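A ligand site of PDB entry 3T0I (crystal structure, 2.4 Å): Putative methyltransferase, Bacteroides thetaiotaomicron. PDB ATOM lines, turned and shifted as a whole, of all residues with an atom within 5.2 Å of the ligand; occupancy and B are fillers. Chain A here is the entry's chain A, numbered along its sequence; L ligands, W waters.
The backbone carbonyl oxygen (O) of Gly 128 lies close to a sulfur (S1) of the ligand (3.7 Å).
Residues that only touch the ligand: Cys 61 (3.4 Å), Gly 62 (3.3 Å), Phe 87 (3.6 Å), Gly 109 (3.5 Å), Ser 110 (3.5 Å) and Ala 129 (3.6 Å).
17 residues have an atom within 4 Å of the ligand: Arg 31, Gln 32, Gly 33, Gly 60, Cys 61, Gly 62, Gln 66, Asp 82, Leu 83, Phe 87, Gly 109, Ser 110, Met 111, Glu 127, Gly 128, Ala 129 and Asn 132.
N of Cys 61 is in hydrogen-bond range of O of Ile 81 (3.3 Å).
The backbone carbonyl oxygen (O) of Asp 82 sits at hydrogen-bond distance from the backbone NH (N) of Gly 109 (2.9 Å).
The guanidinium group (NE) of Arg 31 is in hydrogen-bond range of the side-chain amide oxygen (OE1) of Gln 66 (3.4 Å).
The side-chain amide nitrogen (NE2) of Gln 66 lies within hydrogen-bond range of the backbone carbonyl oxygen (O) of Cys 61 (3.1 Å).
OG of Ser 110 lies within hydrogen-bond range of OD1 of Asp 112 (2.7 Å).
The backbone NH of Gly 60 sits at hydrogen-bond distance from the backbone carbonyl oxygen of Ile 81 (2.6 Å).
The side-chain carboxylate of Asp 82 is in hydrogen-bond range of the backbone NH of Gly 62.
O of Ala 129 sits close to OD1 of Asn 132, at 2.9 Å.
An oxygen (O2) of the ligand is in salt-bridge range of the guanidinium group (NE) of Arg 31 (2.9 Å).
The backbone carbonyl oxygen (O) of Gly 60 lies within hydrogen-bond range of a nitrogen (N1) of the ligand.
ND2 of Asn 132 sits close to N3 of the ligand (3.4 Å).
A nitrogen (N5) of the ligand sits at hydrogen-bond distance from the backbone NH of Met 111, at 2.8 Å.
A nitrogen (N6) of the ligand is in hydrogen-bond range of the backbone NH (N) of Leu 83 (3.2 Å).
The backbone NH (N) of Gly 33 is in hydrogen-bond range of an oxygen (O2) of the ligand (3.3 Å).
The backbone NH of Gln 32 sits at hydrogen-bond distance from an oxygen (O2) of the ligand, at 3.0 Å.
The side-chain amide oxygen of Gln 66 lies close to an oxygen (O2) of the ligand (3.2 Å).
A nitrogen (N1) of the ligand sits at hydrogen-bond distance from the backbone carbonyl oxygen (O) of Glu 127, at 2.9 Å.
O4 of the ligand is in hydrogen-bond range of OD1 of Asp 82, 2.5 Å away.
Water W2 lies within hydrogen-bond range of the side-chain amide oxygen of Gln 32 (2.7 Å), an oxygen (O2) of the ligand (2.9 Å) and the side-chain amide oxygen of Gln 66 (3.2 Å).
Water W1 lies within hydrogen-bond range of N of Glu 127 (2.7 Å), O of Ile 59 (3.0 Å) and N1 of the ligand (3.1 Å).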
ATOM      1  N   ARG A  31      -2.025  -0.389  10.247  1.00  0.00           N
ATOM      2  CA  ARG A  31      -2.977   0.290  11.123  1.00  0.00           C
ATOM      3  C   ARG A  31      -4.333  -0.397  11.080  1.00  0.00           C
ATOM      4  O   ARG A  31      -4.806  -0.829  10.037  1.00  0.00           O
ATOM      5  CB  ARG A  31      -3.157   1.768  10.708  1.00  0.00           C
ATOM      6  CG  ARG A  31      -1.971   2.671  11.010  1.00  0.00           C
ATOM      7  CD  ARG A  31      -1.667   2.715  12.480  1.00  0.00           C
ATOM      8  NE  ARG A  31      -2.743   3.307  13.275  1.00  0.00           N
ATOM      9  CZ  ARG A  31      -2.926   4.616  13.434  1.00  0.00           C
ATOM     10  NH1 ARG A  31      -2.118   5.491  12.853  1.00  0.00           N
ATOM     11  NH2 ARG A  31      -3.923   5.061  14.195  1.00  0.00           N
ATOM     12  N   GLN A  32      -4.970  -0.490  12.245  1.00  0.00           N
ATOM     13  CA  GLN A  32      -6.277  -1.110  12.333  1.00  0.00           C
ATOM     14  C   GLN A  32      -7.371  -0.063  12.423  1.00  0.00           C
ATOM     15  O   GLN A  32      -8.537  -0.389  12.620  1.00  0.00           O
ATOM     16  CB  GLN A  32      -6.352  -2.037  13.552  1.00  0.00           C
ATOM     17  CG  GLN A  32      -5.489  -3.290  13.454  1.00  0.00           C
ATOM     18  CD  GLN A  32      -3.988  -3.005  13.472  1.00  0.00           C
ATOM     19  OE1 GLN A  32      -3.474  -2.379  14.400  1.00  0.00           O
ATOM     20  NE2 GLN A  32      -3.283  -3.490  12.455  1.00  0.00           N
ATOM     21  N   GLY A  33      -6.987   1.205  12.269  1.00  0.00           N
ATOM     22  CA  GLY A  33      -7.963   2.279  12.320  1.00  0.00           C
ATOM     23  C   GLY A  33      -7.444   3.561  11.685  1.00  0.00           C
ATOM     24  O   GLY A  33      -6.239   3.701  11.468  1.00  0.00           O
ATOM     25  N   PRO A  34      -8.322   4.523  11.381  1.00  0.00           N
ATOM     26  CA  PRO A  34      -7.909   5.789  10.768  1.00  0.00           C
ATOM     27  C   PRO A  34      -6.895   6.549  11.628  1.00  0.00           C
ATOM     28  O   PRO A  34      -6.956   6.499  12.854  1.00  0.00           O
ATOM     29  CB  PRO A  34      -9.239   6.545  10.626  1.00  0.00           C
ATOM     30  CG  PRO A  34     -10.230   5.448  10.433  1.00  0.00           C
ATOM     31  CD  PRO A  34      -9.793   4.447  11.482  1.00  0.00           C
ATOM     32  N   ILE A  59      -4.022   2.336  24.992  1.00  0.00           N
ATOM     33  CA  ILE A  59      -5.118   1.374  25.108  1.00  0.00           C
ATOM     34  C   ILE A  59      -5.780   1.049  23.768  1.00  0.00           C
ATOM     35  O   ILE A  59      -6.222   1.947  23.055  1.00  0.00           O
ATOM     36  CB  ILE A  59      -6.165   1.895  26.104  1.00  0.00           C
ATOM     37  CG1 ILE A  59      -5.443   2.310  27.393  1.00  0.00           C
ATOM     38  CG2 ILE A  59      -7.198   0.825  26.425  1.00  0.00           C
ATOM     39  CD1 ILE A  59      -6.305   3.061  28.346  1.00  0.00           C
ATOM     40  N   GLY A  60      -5.865  -0.246  23.458  1.00  0.00           N
ATOM     41  CA  GLY A  60      -6.455  -0.669  22.206  1.00  0.00           C
ATOM     42  C   GLY A  60      -5.447  -0.392  21.102  1.00  0.00           C
ATOM     43  O   GLY A  60      -5.812  -0.109  19.962  1.00  0.00           O
ATOM     44  N   CYS A  61      -4.171  -0.504  21.460  1.00  0.00           N
ATOM     45  CA  CYS A  61      -3.043  -0.266  20.569  1.00  0.00           C
ATOM     46  C   CYS A  61      -3.033  -1.077  19.279  1.00  0.00           C
ATOM     47  O   CYS A  61      -2.376  -0.688  18.308  1.00  0.00           O
ATOM     48  CB  CYS A  61      -1.727  -0.519  21.315  1.00  0.00           C
ATOM     49  SG  CYS A  61      -1.505  -2.238  21.897  1.00  0.00           S
ATOM     50  N   GLY A  62      -3.750  -2.203  19.253  1.00  0.00           N
ATOM     51  CA  GLY A  62      -3.762  -3.031  18.060  1.00  0.00           C
ATOM     52  C   GLY A  62      -2.357  -3.546  17.829  1.00  0.00           C
ATOM     53  O   GLY A  62      -1.715  -4.038  18.768  1.00  0.00           O
ATOM     54  N   GLN A  66       0.366   3.220  15.676  1.00  0.00           N
ATOM     55  CA  GLN A  66       0.418   4.576  16.202  1.00  0.00           C
ATOM     56  C   GLN A  66       1.280   4.661  17.456  1.00  0.00           C
ATOM     57  O   GLN A  66       1.746   5.728  17.840  1.00  0.00           O
ATOM     58  CB  GLN A  66      -0.991   5.114  16.487  1.00  0.00           C
ATOM     59  CG  GLN A  66      -1.714   4.538  17.723  1.00  0.00           C
ATOM     60  CD  GLN A  66      -2.002   3.048  17.615  1.00  0.00           C
ATOM     61  OE1 GLN A  66      -2.318   2.545  16.530  1.00  0.00           O
ATOM     62  NE2 GLN A  66      -1.888   2.334  18.729  1.00  0.00           N
ATOM     63  N   ILE A  81      -1.620  -1.960  25.325  1.00  0.00           N
ATOM     64  CA  ILE A  81      -2.603  -2.920  25.821  1.00  0.00           C
ATOM     65  C   ILE A  81      -3.694  -3.135  24.776  1.00  0.00           C
ATOM     66  O   ILE A  81      -4.274  -2.192  24.250  1.00  0.00           O
ATOM     67  CB  ILE A  81      -3.269  -2.430  27.121  1.00  0.00           C
ATOM     68  CG1 ILE A  81      -2.201  -2.228  28.190  1.00  0.00           C
ATOM     69  CG2 ILE A  81      -4.299  -3.459  27.572  1.00  0.00           C
ATOM     70  CD1 ILE A  81      -2.755  -1.790  29.506  1.00  0.00           C
ATOM     71  N   ASP A  82      -3.967  -4.405  24.494  1.00  0.00           N
ATOM     72  CA  ASP A  82      -4.980  -4.781  23.517  1.00  0.00           C
ATOM     73  C   ASP A  82      -5.559  -6.123  23.914  1.00  0.00           C
ATOM     74  O   ASP A  82      -4.915  -6.934  24.582  1.00  0.00           O
ATOM     75  CB  ASP A  82      -4.366  -4.856  22.127  1.00  0.00           C
ATOM     76  CG  ASP A  82      -5.424  -4.874  21.032  1.00  0.00           C
ATOM     77  OD1 ASP A  82      -6.037  -3.834  20.759  1.00  0.00           O
ATOM     78  OD2 ASP A  82      -5.631  -5.949  20.441  1.00  0.00           O
ATOM     79  N   LEU A  83      -6.810  -6.351  23.523  1.00  0.00           N
ATOM     80  CA  LEU A  83      -7.481  -7.590  23.882  1.00  0.00           C
ATOM     81  C   LEU A  83      -7.050  -8.812  23.061  1.00  0.00           C
ATOM     82  O   LEU A  83      -7.067  -9.948  23.562  1.00  0.00           O
ATOM     83  CB  LEU A  83      -9.005  -7.423  23.767  1.00  0.00           C
ATOM     84  CG  LEU A  83      -9.895  -8.564  24.268  1.00  0.00           C
ATOM     85  CD1 LEU A  83      -9.860  -8.627  25.798  1.00  0.00           C
ATOM     86  CD2 LEU A  83     -11.321  -8.328  23.781  1.00  0.00           C
ATOM     87  N   PHE A  84      -6.648  -8.570  21.811  1.00  0.00           N
ATOM     88  CA  PHE A  84      -6.235  -9.634  20.890  1.00  0.00           C
ATOM     89  C   PHE A  84      -4.743  -9.942  20.997  1.00  0.00           C
ATOM     90  O   PHE A  84      -3.915  -9.173  20.515  1.00  0.00           O
ATOM     91  CB  PHE A  84      -6.575  -9.203  19.463  1.00  0.00           C
ATOM     92  CG  PHE A  84      -6.492 -10.310  18.453  1.00  0.00           C
ATOM     93  CD1 PHE A  84      -7.101 -11.537  18.692  1.00  0.00           C
ATOM     94  CD2 PHE A  84      -5.843 -10.111  17.230  1.00  0.00           C
ATOM     95  CE1 PHE A  84      -7.069 -12.559  17.737  1.00  0.00           C
ATOM     96  CE2 PHE A  84      -5.800 -11.129  16.267  1.00  0.00           C
ATOM     97  CZ  PHE A  84      -6.418 -12.352  16.520  1.00  0.00           C
ATOM     98  N   PHE A  87      -2.242  -9.525  18.109  1.00  0.00           N
ATOM     99  CA  PHE A  87      -1.816  -8.148  17.817  1.00  0.00           C
ATOM    100  C   PHE A  87      -0.622  -7.772  18.669  1.00  0.00           C
ATOM    101  O   PHE A  87       0.296  -7.102  18.203  1.00  0.00           O
ATOM    102  CB  PHE A  87      -2.943  -7.128  18.069  1.00  0.00           C
ATOM    103  CG  PHE A  87      -4.020  -7.099  17.019  1.00  0.00           C
ATOM    104  CD1 PHE A  87      -3.814  -7.677  15.764  1.00  0.00           C
ATOM    105  CD2 PHE A  87      -5.250  -6.488  17.269  1.00  0.00           C
ATOM    106  CE1 PHE A  87      -4.804  -7.634  14.785  1.00  0.00           C
ATOM    107  CE2 PHE A  87      -6.250  -6.443  16.290  1.00  0.00           C
ATOM    108  CZ  PHE A  87      -6.021  -7.016  15.055  1.00  0.00           C
ATOM    109  N   GLY A 109      -4.682  -7.361  27.394  1.00  0.00           N
ATOM    110  CA  GLY A 109      -5.448  -6.931  28.537  1.00  0.00           C
ATOM    111  C   GLY A 109      -6.801  -6.425  28.108  1.00  0.00           C
ATOM    112  O   GLY A 109      -7.050  -6.257  26.913  1.00  0.00           O
ATOM    113  N   SER A 110      -7.684  -6.179  29.076  1.00  0.00           N
ATOM    114  CA  SER A 110      -9.014  -5.679  28.782  1.00  0.00           C
ATOM    115  C   SER A 110      -9.141  -4.195  29.164  1.00  0.00           C
ATOM    116  O   SER A 110      -8.562  -3.738  30.141  1.00  0.00           O
ATOM    117  CB  SER A 110     -10.053  -6.502  29.520  1.00  0.00           C
ATOM    118  OG  SER A 110     -11.355  -6.095  29.138  1.00  0.00           O
ATOM    119  N   MET A 111      -9.924  -3.483  28.367  1.00  0.00           N
ATOM    120  CA  MET A 111     -10.172  -2.056  28.528  1.00  0.00           C
ATOM    121  C   MET A 111     -10.895  -1.679  29.826  1.00  0.00           C
ATOM    122  O   MET A 111     -10.714  -0.578  30.357  1.00  0.00           O
ATOM    123  CB  MET A 111     -10.980  -1.590  27.323  1.00  0.00           C
ATOM    124  CG  MET A 111     -10.660  -0.208  26.857  1.00  0.00           C
ATOM    125  SD  MET A 111     -11.357   0.024  25.235  1.00  0.00           S
ATOM    126  CE  MET A 111      -9.993  -0.540  24.227  1.00  0.00           C
ATOM    127  N   ASP A 112     -11.731  -2.581  30.334  1.00  0.00           N
ATOM    128  CA  ASP A 112     -12.454  -2.337  31.571  1.00  0.00           C
ATOM    129  C   ASP A 112     -11.746  -2.927  32.784  1.00  0.00           C
ATOM    130  O   ASP A 112     -12.316  -2.989  33.869  1.00  0.00           O
ATOM    131  CB  ASP A 112     -13.876  -2.901  31.472  1.00  0.00           C
ATOM    132  CG  ASP A 112     -13.891  -4.381  31.098  1.00  0.00           C
ATOM    133  OD1 ASP A 112     -12.826  -5.027  31.148  1.00  0.00           O
ATOM    134  OD2 ASP A 112     -14.979  -4.892  30.773  1.00  0.00           O
ATOM    135  N   GLU A 127      -6.189   5.371  20.215  1.00  0.00           N
ATOM    136  CA  GLU A 127      -6.706   5.773  18.916  1.00  0.00           C
ATOM    137  C   GLU A 127      -7.752   4.791  18.389  1.00  0.00           C
ATOM    138  O   GLU A 127      -7.501   3.594  18.297  1.00  0.00           O
ATOM    139  CB  GLU A 127      -5.548   5.931  17.921  1.00  0.00           C
ATOM    140  CG  GLU A 127      -4.521   6.978  18.369  1.00  0.00           C
ATOM    141  CD  GLU A 127      -3.650   7.515  17.237  1.00  0.00           C
ATOM    142  OE1 GLU A 127      -2.626   8.155  17.548  1.00  0.00           O
ATOM    143  OE2 GLU A 127      -3.983   7.309  16.055  1.00  0.00           O
ATOM    144  N   GLY A 128      -8.923   5.319  18.076  1.00  0.00           N
ATOM    145  CA  GLY A 128     -10.009   4.516  17.562  1.00  0.00           C
ATOM    146  C   GLY A 128     -10.252   3.218  18.312  1.00  0.00           C
ATOM    147  O   GLY A 128     -10.453   2.173  17.681  1.00  0.00           O
ATOM    148  N   ALA A 129     -10.254   3.286  19.633  1.00  0.00           N
ATOM    149  CA  ALA A 129     -10.472   2.088  20.447  1.00  0.00           C
ATOM    150  C   ALA A 129     -11.387   2.303  21.649  1.00  0.00           C
ATOM    151  O   ALA A 129     -12.007   1.364  22.135  1.00  0.00           O
ATOM    152  CB  ALA A 129      -9.130   1.530  20.911  1.00  0.00           C
ATOM    153  N   TYR A 131     -14.202   3.398  21.808  1.00  0.00           N
ATOM    154  CA  TYR A 131     -15.579   3.061  21.483  1.00  0.00           C
ATOM    155  C   TYR A 131     -15.974   1.699  22.065  1.00  0.00           C
ATOM    156  O   TYR A 131     -17.154   1.437  22.332  1.00  0.00           O
ATOM    157  CB  TYR A 131     -15.798   3.080  19.970  1.00  0.00           C
ATOM    158  CG  TYR A 131     -15.181   1.902  19.232  1.00  0.00           C
ATOM    159  CD1 TYR A 131     -15.831   0.659  19.204  1.00  0.00           C
ATOM    160  CD2 TYR A 131     -13.959   2.030  18.573  1.00  0.00           C
ATOM    161  CE1 TYR A 131     -15.263  -0.426  18.528  1.00  0.00           C
ATOM    162  CE2 TYR A 131     -13.398   0.956  17.902  1.00  0.00           C
ATOM    163  CZ  TYR A 131     -14.044  -0.266  17.879  1.00  0.00           C
ATOM    164  OH  TYR A 131     -13.479  -1.325  17.220  1.00  0.00           O
ATOM    165  N   ASN A 132     -14.975   0.832  22.256  1.00  0.00           N
ATOM    166  CA  ASN A 132     -15.233  -0.510  22.784  1.00  0.00           C
ATOM    167  C   ASN A 132     -15.811  -0.511  24.211  1.00  0.00           C
ATOM    168  O   ASN A 132     -16.346  -1.520  24.645  1.00  0.00           O
ATOM    169  CB  ASN A 132     -13.959  -1.357  22.728  1.00  0.00           C
ATOM    170  CG  ASN A 132     -13.555  -1.720  21.297  1.00  0.00           C
ATOM    171  OD1 ASN A 132     -12.796  -1.006  20.640  1.00  0.00           O
ATOM    172  ND2 ASN A 132     -14.078  -2.843  20.802  1.00  0.00           N
HETATM  173  N1  LIG L   1      -5.341   1.704  18.012  1.00  0.00           N
HETATM  174  C1  LIG L   1      -5.050   0.903  16.819  1.00  0.00           C
HETATM  175  C2  LIG L   1      -6.128  -0.173  16.642  1.00  0.00           C
HETATM  176  C3  LIG L   1      -7.529   0.439  16.595  1.00  0.00           C
HETATM  177  S1  LIG L   1      -8.843  -0.806  16.313  1.00  0.00           S
HETATM  178  C4  LIG L   1      -5.019   1.818  15.597  1.00  0.00           C
HETATM  179  O1  LIG L   1      -5.479   2.985  15.763  1.00  0.00           O
HETATM  180  O2  LIG L   1      -4.553   1.367  14.546  1.00  0.00           O
HETATM  181  C5  LIG L   1      -9.512  -1.011  18.002  1.00  0.00           C
HETATM  182  C6  LIG L   1      -8.615  -1.823  18.942  1.00  0.00           C
HETATM  183  O3  LIG L   1      -9.290  -2.006  20.185  1.00  0.00           O
HETATM  184  C7  LIG L   1      -8.363  -3.231  18.371  1.00  0.00           C
HETATM  185  O4  LIG L   1      -6.970  -3.520  18.453  1.00  0.00           O
HETATM  186  C8  LIG L   1      -9.164  -4.119  19.318  1.00  0.00           C
HETATM  187  O5  LIG L   1      -8.525  -5.392  19.435  1.00  0.00           O
HETATM  188  C9  LIG L   1      -8.965  -3.338  20.615  1.00  0.00           C
HETATM  189  N2  LIG L   1      -9.901  -3.791  21.674  1.00  0.00           N
HETATM  190  C10 LIG L   1     -11.179  -4.119  21.506  1.00  0.00           C
HETATM  191  N3  LIG L   1     -11.739  -4.373  22.688  1.00  0.00           N
HETATM  192  C11 LIG L   1     -10.817  -4.211  23.621  1.00  0.00           C
HETATM  193  C12 LIG L   1     -10.813  -4.310  25.007  1.00  0.00           C
HETATM  194  N4  LIG L   1     -11.917  -4.641  25.659  1.00  0.00           N
HETATM  195  N5  LIG L   1      -9.662  -4.055  25.679  1.00  0.00           N
HETATM  196  C13 LIG L   1      -8.568  -3.722  25.027  1.00  0.00           C
HETATM  197  N6  LIG L   1      -8.536  -3.613  23.702  1.00  0.00           N
HETATM  198  C14 LIG L   1      -9.633  -3.845  22.982  1.00  0.00           C
HETATM  199  O   HOH W   1      -4.762   3.187  20.699  1.00  0.00           O
HETATM  200  O   HOH W   2      -2.004  -0.081  14.715  1.00  0.00           O
